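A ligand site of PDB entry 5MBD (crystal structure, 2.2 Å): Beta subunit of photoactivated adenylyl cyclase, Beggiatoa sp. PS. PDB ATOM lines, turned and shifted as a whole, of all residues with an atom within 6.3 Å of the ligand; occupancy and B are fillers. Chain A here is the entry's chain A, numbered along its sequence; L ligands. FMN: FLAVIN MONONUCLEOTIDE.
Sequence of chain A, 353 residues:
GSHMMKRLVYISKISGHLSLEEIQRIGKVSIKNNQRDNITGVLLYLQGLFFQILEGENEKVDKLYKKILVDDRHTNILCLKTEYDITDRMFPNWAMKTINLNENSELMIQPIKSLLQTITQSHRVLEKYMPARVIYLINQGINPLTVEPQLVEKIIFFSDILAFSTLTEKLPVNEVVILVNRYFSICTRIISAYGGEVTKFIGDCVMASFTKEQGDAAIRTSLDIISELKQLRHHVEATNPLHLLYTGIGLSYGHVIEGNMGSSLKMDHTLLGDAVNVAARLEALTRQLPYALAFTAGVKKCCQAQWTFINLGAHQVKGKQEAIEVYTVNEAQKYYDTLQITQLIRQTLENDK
The guanidinium group of Arg 73 is in salt-bridge range of the side-chain carboxylate of Asp 71 (2.8 Å). O of Asn 34 is in hydrogen-bond range of N of Ile 39 (3.0 Å). ND2 of Asn 34 lies within hydrogen-bond range of O of Ala 95. ND2 of Asn 33 sits at hydrogen-bond distance from O of Val 29. The backbone carbonyl oxygen of Ser 12 lies within hydrogen-bond range of the backbone NH of Phe 50. N of Leu 43 lies within hydrogen-bond range of SD of Met 96, 3.3 Å away. The backbone carbonyl oxygen (O) of Ile 68 is in hydrogen-bond range of a ring nitrogen (NE2) of His 74 (2.9 Å). ND1 of His 74 sits at hydrogen-bond distance from OG of Ser 12 (2.8 Å).
Merely in contact with the ligand: Leu 64, Asn 33, Phe 50, Asp 71, Met 96, Tyr 10, Ile 68, Ile 26, His 74, Leu 43 and Leu 54. Within 4 Å of the ligand: Tyr 10, Ile 26, Ser 30, Asn 33, Asn 34, Leu 43, Phe 50, Gln 52, Leu 54, Leu 64, Lys 67, Ile 68, Asp 71, Arg 73, His 74 and Met 96. The nearest printed residue that does not touch the ligand is Val 29 (4.3 Å).
The guanidinium group (NH2) of Arg 73 is in hydrogen-bond range of an oxygen (O4') of the ligand (2.6 Å). O4 of the ligand lies within hydrogen-bond range of NE2 of Gln 52, 2.8 Å away. The side-chain hydroxyl (OG) of Ser 30 lies close to a nitrogen (N5) of the ligand. OD1 of Asn 34 is in hydrogen-bond range of N3 of the ligand. NZ of Lys 67 lies within salt-bridge range of O2P of the ligand (3.3 Å).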
ATOM      1  N   TYR A  10       4.125  28.742   4.384  1.00  0.00           N
ATOM      2  CA  TYR A  10       3.005  28.995   5.281  1.00  0.00           C
ATOM      3  C   TYR A  10       2.647  27.702   5.993  1.00  0.00           C
ATOM      4  O   TYR A  10       3.001  26.604   5.554  1.00  0.00           O
ATOM      5  CB  TYR A  10       1.777  29.556   4.532  1.00  0.00           C
ATOM      6  CG  TYR A  10       0.950  28.523   3.780  1.00  0.00           C
ATOM      7  CD1 TYR A  10      -0.040  27.778   4.430  1.00  0.00           C
ATOM      8  CD2 TYR A  10       1.144  28.315   2.424  1.00  0.00           C
ATOM      9  CE1 TYR A  10      -0.791  26.837   3.746  1.00  0.00           C
ATOM     10  CE2 TYR A  10       0.384  27.386   1.733  1.00  0.00           C
ATOM     11  CZ  TYR A  10      -0.578  26.650   2.393  1.00  0.00           C
ATOM     12  OH  TYR A  10      -1.334  25.719   1.731  1.00  0.00           O
ATOM     13  N   SER A  12      -0.853  25.866   8.234  1.00  0.00           N
ATOM     14  CA  SER A  12      -2.298  25.919   8.446  1.00  0.00           C
ATOM     15  C   SER A  12      -2.744  24.701   9.232  1.00  0.00           C
ATOM     16  O   SER A  12      -2.054  23.690   9.310  1.00  0.00           O
ATOM     17  CB  SER A  12      -3.052  25.999   7.120  1.00  0.00           C
ATOM     18  OG  SER A  12      -2.958  24.762   6.413  1.00  0.00           O
ATOM     19  N   ARG A  25      -5.679  13.307  -2.874  1.00  0.00           N
ATOM     20  CA  ARG A  25      -6.375  14.025  -3.929  1.00  0.00           C
ATOM     21  C   ARG A  25      -5.887  15.463  -4.018  1.00  0.00           C
ATOM     22  O   ARG A  25      -5.759  16.018  -5.123  1.00  0.00           O
ATOM     23  CB  ARG A  25      -7.896  14.001  -3.700  1.00  0.00           C
ATOM     24  CG  ARG A  25      -8.672  14.648  -4.837  1.00  0.00           C
ATOM     25  CD  ARG A  25     -10.182  14.509  -4.706  1.00  0.00           C
ATOM     26  NE  ARG A  25     -10.686  15.128  -3.491  1.00  0.00           N
ATOM     27  CZ  ARG A  25     -11.035  16.408  -3.385  1.00  0.00           C
ATOM     28  NH1 ARG A  25     -10.916  17.225  -4.420  1.00  0.00           N
ATOM     29  NH2 ARG A  25     -11.499  16.868  -2.231  1.00  0.00           N
ATOM     30  N   ILE A  26      -5.614  16.080  -2.868  1.00  0.00           N
ATOM     31  CA  ILE A  26      -4.962  17.394  -2.853  1.00  0.00           C
ATOM     32  C   ILE A  26      -3.630  17.318  -3.596  1.00  0.00           C
ATOM     33  O   ILE A  26      -3.277  18.209  -4.365  1.00  0.00           O
ATOM     34  CB  ILE A  26      -4.760  17.892  -1.410  1.00  0.00           C
ATOM     35  CG1 ILE A  26      -6.084  17.944  -0.641  1.00  0.00           C
ATOM     36  CG2 ILE A  26      -4.109  19.275  -1.407  1.00  0.00           C
ATOM     37  CD1 ILE A  26      -5.914  18.346   0.829  1.00  0.00           C
ATOM     38  N   VAL A  29      -4.264  17.109  -7.576  1.00  0.00           N
ATOM     39  CA  VAL A  29      -4.727  18.357  -8.203  1.00  0.00           C
ATOM     40  C   VAL A  29      -3.596  19.379  -8.253  1.00  0.00           C
ATOM     41  O   VAL A  29      -3.414  20.080  -9.252  1.00  0.00           O
ATOM     42  CB  VAL A  29      -5.995  18.890  -7.511  1.00  0.00           C
ATOM     43  CG1 VAL A  29      -5.746  19.230  -6.036  1.00  0.00           C
ATOM     44  CG2 VAL A  29      -6.578  20.087  -8.272  1.00  0.00           C
ATOM     45  N   SER A  30      -2.780  19.436  -7.193  1.00  0.00           N
ATOM     46  CA  SER A  30      -1.732  20.459  -7.144  1.00  0.00           C
ATOM     47  C   SER A  30      -0.668  20.221  -8.208  1.00  0.00           C
ATOM     48  O   SER A  30      -0.212  21.175  -8.858  1.00  0.00           O
ATOM     49  CB  SER A  30      -1.091  20.496  -5.749  1.00  0.00           C
ATOM     50  OG  SER A  30      -2.081  20.682  -4.746  1.00  0.00           O
ATOM     51  N   ILE A  31      -0.237  18.973  -8.383  1.00  0.00           N
ATOM     52  CA  ILE A  31       0.723  18.622  -9.436  1.00  0.00           C
ATOM     53  C   ILE A  31       0.261  19.152 -10.785  1.00  0.00           C
ATOM     54  O   ILE A  31       1.016  19.825 -11.508  1.00  0.00           O
ATOM     55  CB  ILE A  31       0.927  17.091  -9.486  1.00  0.00           C
ATOM     56  CG1 ILE A  31       1.531  16.579  -8.168  1.00  0.00           C
ATOM     57  CG2 ILE A  31       1.783  16.673 -10.677  1.00  0.00           C
ATOM     58  CD1 ILE A  31       1.628  15.056  -8.069  1.00  0.00           C
ATOM     59  N   ASN A  33      -2.120  21.537 -11.731  1.00  0.00           N
ATOM     60  CA  ASN A  33      -2.158  22.987 -11.847  1.00  0.00           C
ATOM     61  C   ASN A  33      -0.763  23.606 -11.746  1.00  0.00           C
ATOM     62  O   ASN A  33      -0.457  24.568 -12.464  1.00  0.00           O
ATOM     63  CB  ASN A  33      -3.092  23.576 -10.784  1.00  0.00           C
ATOM     64  CG  ASN A  33      -4.576  23.293 -11.063  1.00  0.00           C
ATOM     65  OD1 ASN A  33      -5.194  23.889 -11.944  1.00  0.00           O
ATOM     66  ND2 ASN A  33      -5.156  22.387 -10.282  1.00  0.00           N
ATOM     67  N   ASN A  34       0.092  23.068 -10.877  1.00  0.00           N
ATOM     68  CA  ASN A  34       1.418  23.661 -10.709  1.00  0.00           C
ATOM     69  C   ASN A  34       2.313  23.371 -11.907  1.00  0.00           C
ATOM     70  O   ASN A  34       3.155  24.209 -12.282  1.00  0.00           O
ATOM     71  CB  ASN A  34       2.083  23.168  -9.410  1.00  0.00           C
ATOM     72  CG  ASN A  34       1.393  23.704  -8.160  1.00  0.00           C
ATOM     73  OD1 ASN A  34       0.738  24.745  -8.190  1.00  0.00           O
ATOM     74  ND2 ASN A  34       1.545  22.981  -7.054  1.00  0.00           N
ATOM     75  N   ILE A  39       5.019  26.265 -11.207  1.00  0.00           N
ATOM     76  CA  ILE A  39       5.107  26.383  -9.762  1.00  0.00           C
ATOM     77  C   ILE A  39       5.658  25.071  -9.229  1.00  0.00           C
ATOM     78  O   ILE A  39       5.132  23.992  -9.531  1.00  0.00           O
ATOM     79  CB  ILE A  39       3.741  26.697  -9.135  1.00  0.00           C
ATOM     80  CG1 ILE A  39       3.317  28.131  -9.453  1.00  0.00           C
ATOM     81  CG2 ILE A  39       3.755  26.445  -7.627  1.00  0.00           C
ATOM     82  CD1 ILE A  39       1.884  28.429  -9.058  1.00  0.00           C
ATOM     83  N   LEU A  43       4.427  20.025  -0.285  1.00  0.00           N
ATOM     84  CA  LEU A  43       3.331  19.993   0.665  1.00  0.00           C
ATOM     85  C   LEU A  43       3.599  18.910   1.708  1.00  0.00           C
ATOM     86  O   LEU A  43       3.964  17.791   1.360  1.00  0.00           O
ATOM     87  CB  LEU A  43       1.986  19.739  -0.020  1.00  0.00           C
ATOM     88  CG  LEU A  43       0.826  19.584   0.972  1.00  0.00           C
ATOM     89  CD1 LEU A  43       0.507  20.896   1.670  1.00  0.00           C
ATOM     90  CD2 LEU A  43      -0.408  19.014   0.275  1.00  0.00           C
ATOM     91  N   PHE A  50      -0.654  21.538   8.253  1.00  0.00           N
ATOM     92  CA  PHE A  50      -0.182  21.595   6.876  1.00  0.00           C
ATOM     93  C   PHE A  50       1.011  22.549   6.803  1.00  0.00           C
ATOM     94  O   PHE A  50       0.950  23.664   7.331  1.00  0.00           O
ATOM     95  CB  PHE A  50      -1.288  22.076   5.936  1.00  0.00           C
ATOM     96  CG  PHE A  50      -2.128  20.963   5.354  1.00  0.00           C
ATOM     97  CD1 PHE A  50      -1.532  19.812   4.880  1.00  0.00           C
ATOM     98  CD2 PHE A  50      -3.518  21.080   5.288  1.00  0.00           C
ATOM     99  CE1 PHE A  50      -2.293  18.794   4.343  1.00  0.00           C
ATOM    100  CE2 PHE A  50      -4.282  20.052   4.741  1.00  0.00           C
ATOM    101  CZ  PHE A  50      -3.665  18.910   4.271  1.00  0.00           C
ATOM    102  N   GLN A  52       3.464  24.099   3.657  1.00  0.00           N
ATOM    103  CA  GLN A  52       3.642  24.143   2.226  1.00  0.00           C
ATOM    104  C   GLN A  52       4.666  25.202   1.836  1.00  0.00           C
ATOM    105  O   GLN A  52       4.674  26.301   2.391  1.00  0.00           O
ATOM    106  CB  GLN A  52       2.324  24.396   1.483  1.00  0.00           C
ATOM    107  CG  GLN A  52       2.458  24.214  -0.018  1.00  0.00           C
ATOM    108  CD  GLN A  52       1.137  24.083  -0.739  1.00  0.00           C
ATOM    109  OE1 GLN A  52       0.193  24.832  -0.469  1.00  0.00           O
ATOM    110  NE2 GLN A  52       1.070  23.145  -1.672  1.00  0.00           N
ATOM    111  N   LEU A  54       6.047  27.148  -1.627  1.00  0.00           N
ATOM    112  CA  LEU A  54       5.629  27.477  -2.984  1.00  0.00           C
ATOM    113  C   LEU A  54       6.619  28.454  -3.572  1.00  0.00           C
ATOM    114  O   LEU A  54       6.962  29.455  -2.932  1.00  0.00           O
ATOM    115  CB  LEU A  54       4.209  28.073  -3.005  1.00  0.00           C
ATOM    116  CG  LEU A  54       3.046  27.122  -2.733  1.00  0.00           C
ATOM    117  CD1 LEU A  54       1.703  27.832  -2.812  1.00  0.00           C
ATOM    118  CD2 LEU A  54       3.097  25.976  -3.724  1.00  0.00           C
ATOM    119  N   LEU A  64      -2.230  31.545  -7.109  1.00  0.00           N
ATOM    120  CA  LEU A  64      -2.519  30.283  -6.431  1.00  0.00           C
ATOM    121  C   LEU A  64      -2.792  30.503  -4.950  1.00  0.00           C
ATOM    122  O   LEU A  64      -3.688  29.868  -4.380  1.00  0.00           O
ATOM    123  CB  LEU A  64      -1.364  29.309  -6.646  1.00  0.00           C
ATOM    124  CG  LEU A  64      -1.280  28.058  -5.748  1.00  0.00           C
ATOM    125  CD1 LEU A  64      -2.538  27.213  -5.881  1.00  0.00           C
ATOM    126  CD2 LEU A  64      -0.033  27.247  -6.069  1.00  0.00           C
ATOM    127  N   LYS A  67      -6.259  31.389  -4.097  1.00  0.00           N
ATOM    128  CA  LYS A  67      -7.108  30.204  -4.187  1.00  0.00           C
ATOM    129  C   LYS A  67      -6.976  29.338  -2.942  1.00  0.00           C
ATOM    130  O   LYS A  67      -7.975  28.813  -2.438  1.00  0.00           O
ATOM    131  CB  LYS A  67      -6.740  29.406  -5.440  1.00  0.00           C
ATOM    132  CG  LYS A  67      -7.558  28.147  -5.682  1.00  0.00           C
ATOM    133  CD  LYS A  67      -8.815  28.455  -6.485  1.00  0.00           C
ATOM    134  CE  LYS A  67      -9.495  27.173  -6.932  1.00  0.00           C
ATOM    135  NZ  LYS A  67     -10.599  27.436  -7.890  1.00  0.00           N
ATOM    136  N   ILE A  68      -5.750  29.183  -2.433  1.00  0.00           N
ATOM    137  CA  ILE A  68      -5.523  28.294  -1.299  1.00  0.00           C
ATOM    138  C   ILE A  68      -6.193  28.838  -0.044  1.00  0.00           C
ATOM    139  O   ILE A  68      -6.768  28.079   0.754  1.00  0.00           O
ATOM    140  CB  ILE A  68      -4.015  28.049  -1.099  1.00  0.00           C
ATOM    141  CG1 ILE A  68      -3.405  27.360  -2.314  1.00  0.00           C
ATOM    142  CG2 ILE A  68      -3.761  27.196   0.129  1.00  0.00           C
ATOM    143  CD1 ILE A  68      -1.952  26.952  -2.147  1.00  0.00           C
ATOM    144  N   ASP A  71      -9.851  27.821   0.392  1.00  0.00           N
ATOM    145  CA  ASP A  71     -10.173  26.407   0.485  1.00  0.00           C
ATOM    146  C   ASP A  71     -10.682  26.066   1.878  1.00  0.00           C
ATOM    147  O   ASP A  71     -10.044  26.378   2.884  1.00  0.00           O
ATOM    148  CB  ASP A  71      -8.945  25.558   0.147  1.00  0.00           C
ATOM    149  CG  ASP A  71      -9.268  24.082   0.081  1.00  0.00           C
ATOM    150  OD1 ASP A  71      -9.717  23.517   1.101  1.00  0.00           O
ATOM    151  OD2 ASP A  71      -9.068  23.469  -0.988  1.00  0.00           O
ATOM    152  N   ARG A  73     -10.740  23.275   3.366  1.00  0.00           N
ATOM    153  CA  ARG A  73     -10.168  22.100   4.036  1.00  0.00           C
ATOM    154  C   ARG A  73      -9.214  22.491   5.155  1.00  0.00           C
ATOM    155  O   ARG A  73      -8.944  21.677   6.044  1.00  0.00           O
ATOM    156  CB  ARG A  73      -9.467  21.201   3.025  1.00  0.00           C
ATOM    157  CG  ARG A  73     -10.419  20.379   2.168  1.00  0.00           C
ATOM    158  CD  ARG A  73      -9.760  19.852   0.893  1.00  0.00           C
ATOM    159  NE  ARG A  73      -9.623  20.861  -0.150  1.00  0.00           N
ATOM    160  CZ  ARG A  73      -9.450  20.583  -1.448  1.00  0.00           C
ATOM    161  NH1 ARG A  73      -9.412  19.328  -1.866  1.00  0.00           N
ATOM    162  NH2 ARG A  73      -9.322  21.577  -2.319  1.00  0.00           N
ATOM    163  N   HIS A  74      -8.708  23.727   5.145  1.00  0.00           N
ATOM    164  CA  HIS A  74      -7.790  24.169   6.186  1.00  0.00           C
ATOM    165  C   HIS A  74      -8.132  25.584   6.639  1.00  0.00           C
ATOM    166  O   HIS A  74      -8.767  26.357   5.921  1.00  0.00           O
ATOM    167  CB  HIS A  74      -6.318  24.075   5.718  1.00  0.00           C
ATOM    168  CG  HIS A  74      -5.978  24.961   4.568  1.00  0.00           C
ATOM    169  ND1 HIS A  74      -4.674  25.178   4.177  1.00  0.00           N
ATOM    170  CD2 HIS A  74      -6.753  25.675   3.713  1.00  0.00           C
ATOM    171  CE1 HIS A  74      -4.656  25.985   3.130  1.00  0.00           C
ATOM    172  NE2 HIS A  74      -5.902  26.302   2.828  1.00  0.00           N
ATOM    173  N   ALA A  95       6.778  19.518  -9.055  1.00  0.00           N
ATOM    174  CA  ALA A  95       5.581  20.347  -9.204  1.00  0.00           C
ATOM    175  C   ALA A  95       4.885  20.539  -7.869  1.00  0.00           C
ATOM    176  O   ALA A  95       4.592  21.670  -7.452  1.00  0.00           O
ATOM    177  CB  ALA A  95       4.641  19.706 -10.230  1.00  0.00           C
ATOM    178  N   MET A  96       4.614  19.430  -7.175  1.00  0.00           N
ATOM    179  CA  MET A  96       4.169  19.483  -5.786  1.00  0.00           C
ATOM    180  C   MET A  96       4.433  18.126  -5.155  1.00  0.00           C
ATOM    181  O   MET A  96       3.694  17.166  -5.421  1.00  0.00           O
ATOM    182  CB  MET A  96       2.697  19.877  -5.682  1.00  0.00           C
ATOM    183  CG  MET A  96       2.200  20.164  -4.261  1.00  0.00           C
ATOM    184  SD  MET A  96       3.335  21.090  -3.213  1.00  0.00           S
ATOM    185  CE  MET A  96       3.584  22.560  -4.199  1.00  0.00           C
HETATM  186  N1  FMN L   1      -3.731  23.789  -5.441  1.00  0.00           N
HETATM  187  C2  FMN L   1      -2.710  23.971  -6.346  1.00  0.00           C
HETATM  188  O2  FMN L   1      -2.982  24.201  -7.526  1.00  0.00           O
HETATM  189  N3  FMN L   1      -1.399  23.908  -5.938  1.00  0.00           N
HETATM  190  C4  FMN L   1      -1.113  23.657  -4.619  1.00  0.00           C
HETATM  191  O4  FMN L   1       0.056  23.595  -4.237  1.00  0.00           O
HETATM  192  C4A FMN L   1      -2.141  23.463  -3.701  1.00  0.00           C
HETATM  193  N5  FMN L   1      -1.814  23.212  -2.388  1.00  0.00           N
HETATM  194  C5A FMN L   1      -2.810  23.020  -1.464  1.00  0.00           C
HETATM  195  C6  FMN L   1      -2.466  22.768  -0.156  1.00  0.00           C
HETATM  196  C7  FMN L   1      -3.458  22.573   0.798  1.00  0.00           C
HETATM  197  C7M FMN L   1      -3.079  22.303   2.215  1.00  0.00           C
HETATM  198  C8  FMN L   1      -4.794  22.627   0.426  1.00  0.00           C
HETATM  199  C8M FMN L   1      -5.873  22.421   1.451  1.00  0.00           C
HETATM  200  C9  FMN L   1      -5.138  22.890  -0.901  1.00  0.00           C
HETATM  201  C9A FMN L   1      -4.137  23.086  -1.849  1.00  0.00           C
HETATM  202  N10 FMN L   1      -4.489  23.337  -3.163  1.00  0.00           N
HETATM  203  C10 FMN L   1      -3.473  23.535  -4.099  1.00  0.00           C
HETATM  204  C1' FMN L   1      -5.977  23.380  -3.458  1.00  0.00           C
HETATM  205  C2' FMN L   1      -6.444  24.398  -4.487  1.00  0.00           C
HETATM  206  O2' FMN L   1      -7.373  25.302  -3.920  1.00  0.00           O
HETATM  207  C3' FMN L   1      -7.075  23.671  -5.672  1.00  0.00           C
HETATM  208  O3' FMN L   1      -6.657  24.263  -6.878  1.00  0.00           O
HETATM  209  C4' FMN L   1      -8.599  23.661  -5.579  1.00  0.00           C
HETATM  210  O4' FMN L   1      -9.016  22.854  -4.508  1.00  0.00           O
HETATM  211  C5' FMN L   1      -9.218  23.154  -6.869  1.00  0.00           C
HETATM  212  O5' FMN L   1      -9.011  24.102  -7.895  1.00  0.00           O
HETATM  213  P   FMN L   1      -9.977  24.129  -9.175  1.00  0.00           P
HETATM  214  O1P FMN L   1     -11.390  24.362  -8.694  1.00  0.00           O
HETATM  215  O2P FMN L   1      -9.569  25.253 -10.099  1.00  0.00           O
HETATM  216  O3P FMN L   1      -9.894  22.807  -9.921  1.00  0.00           O
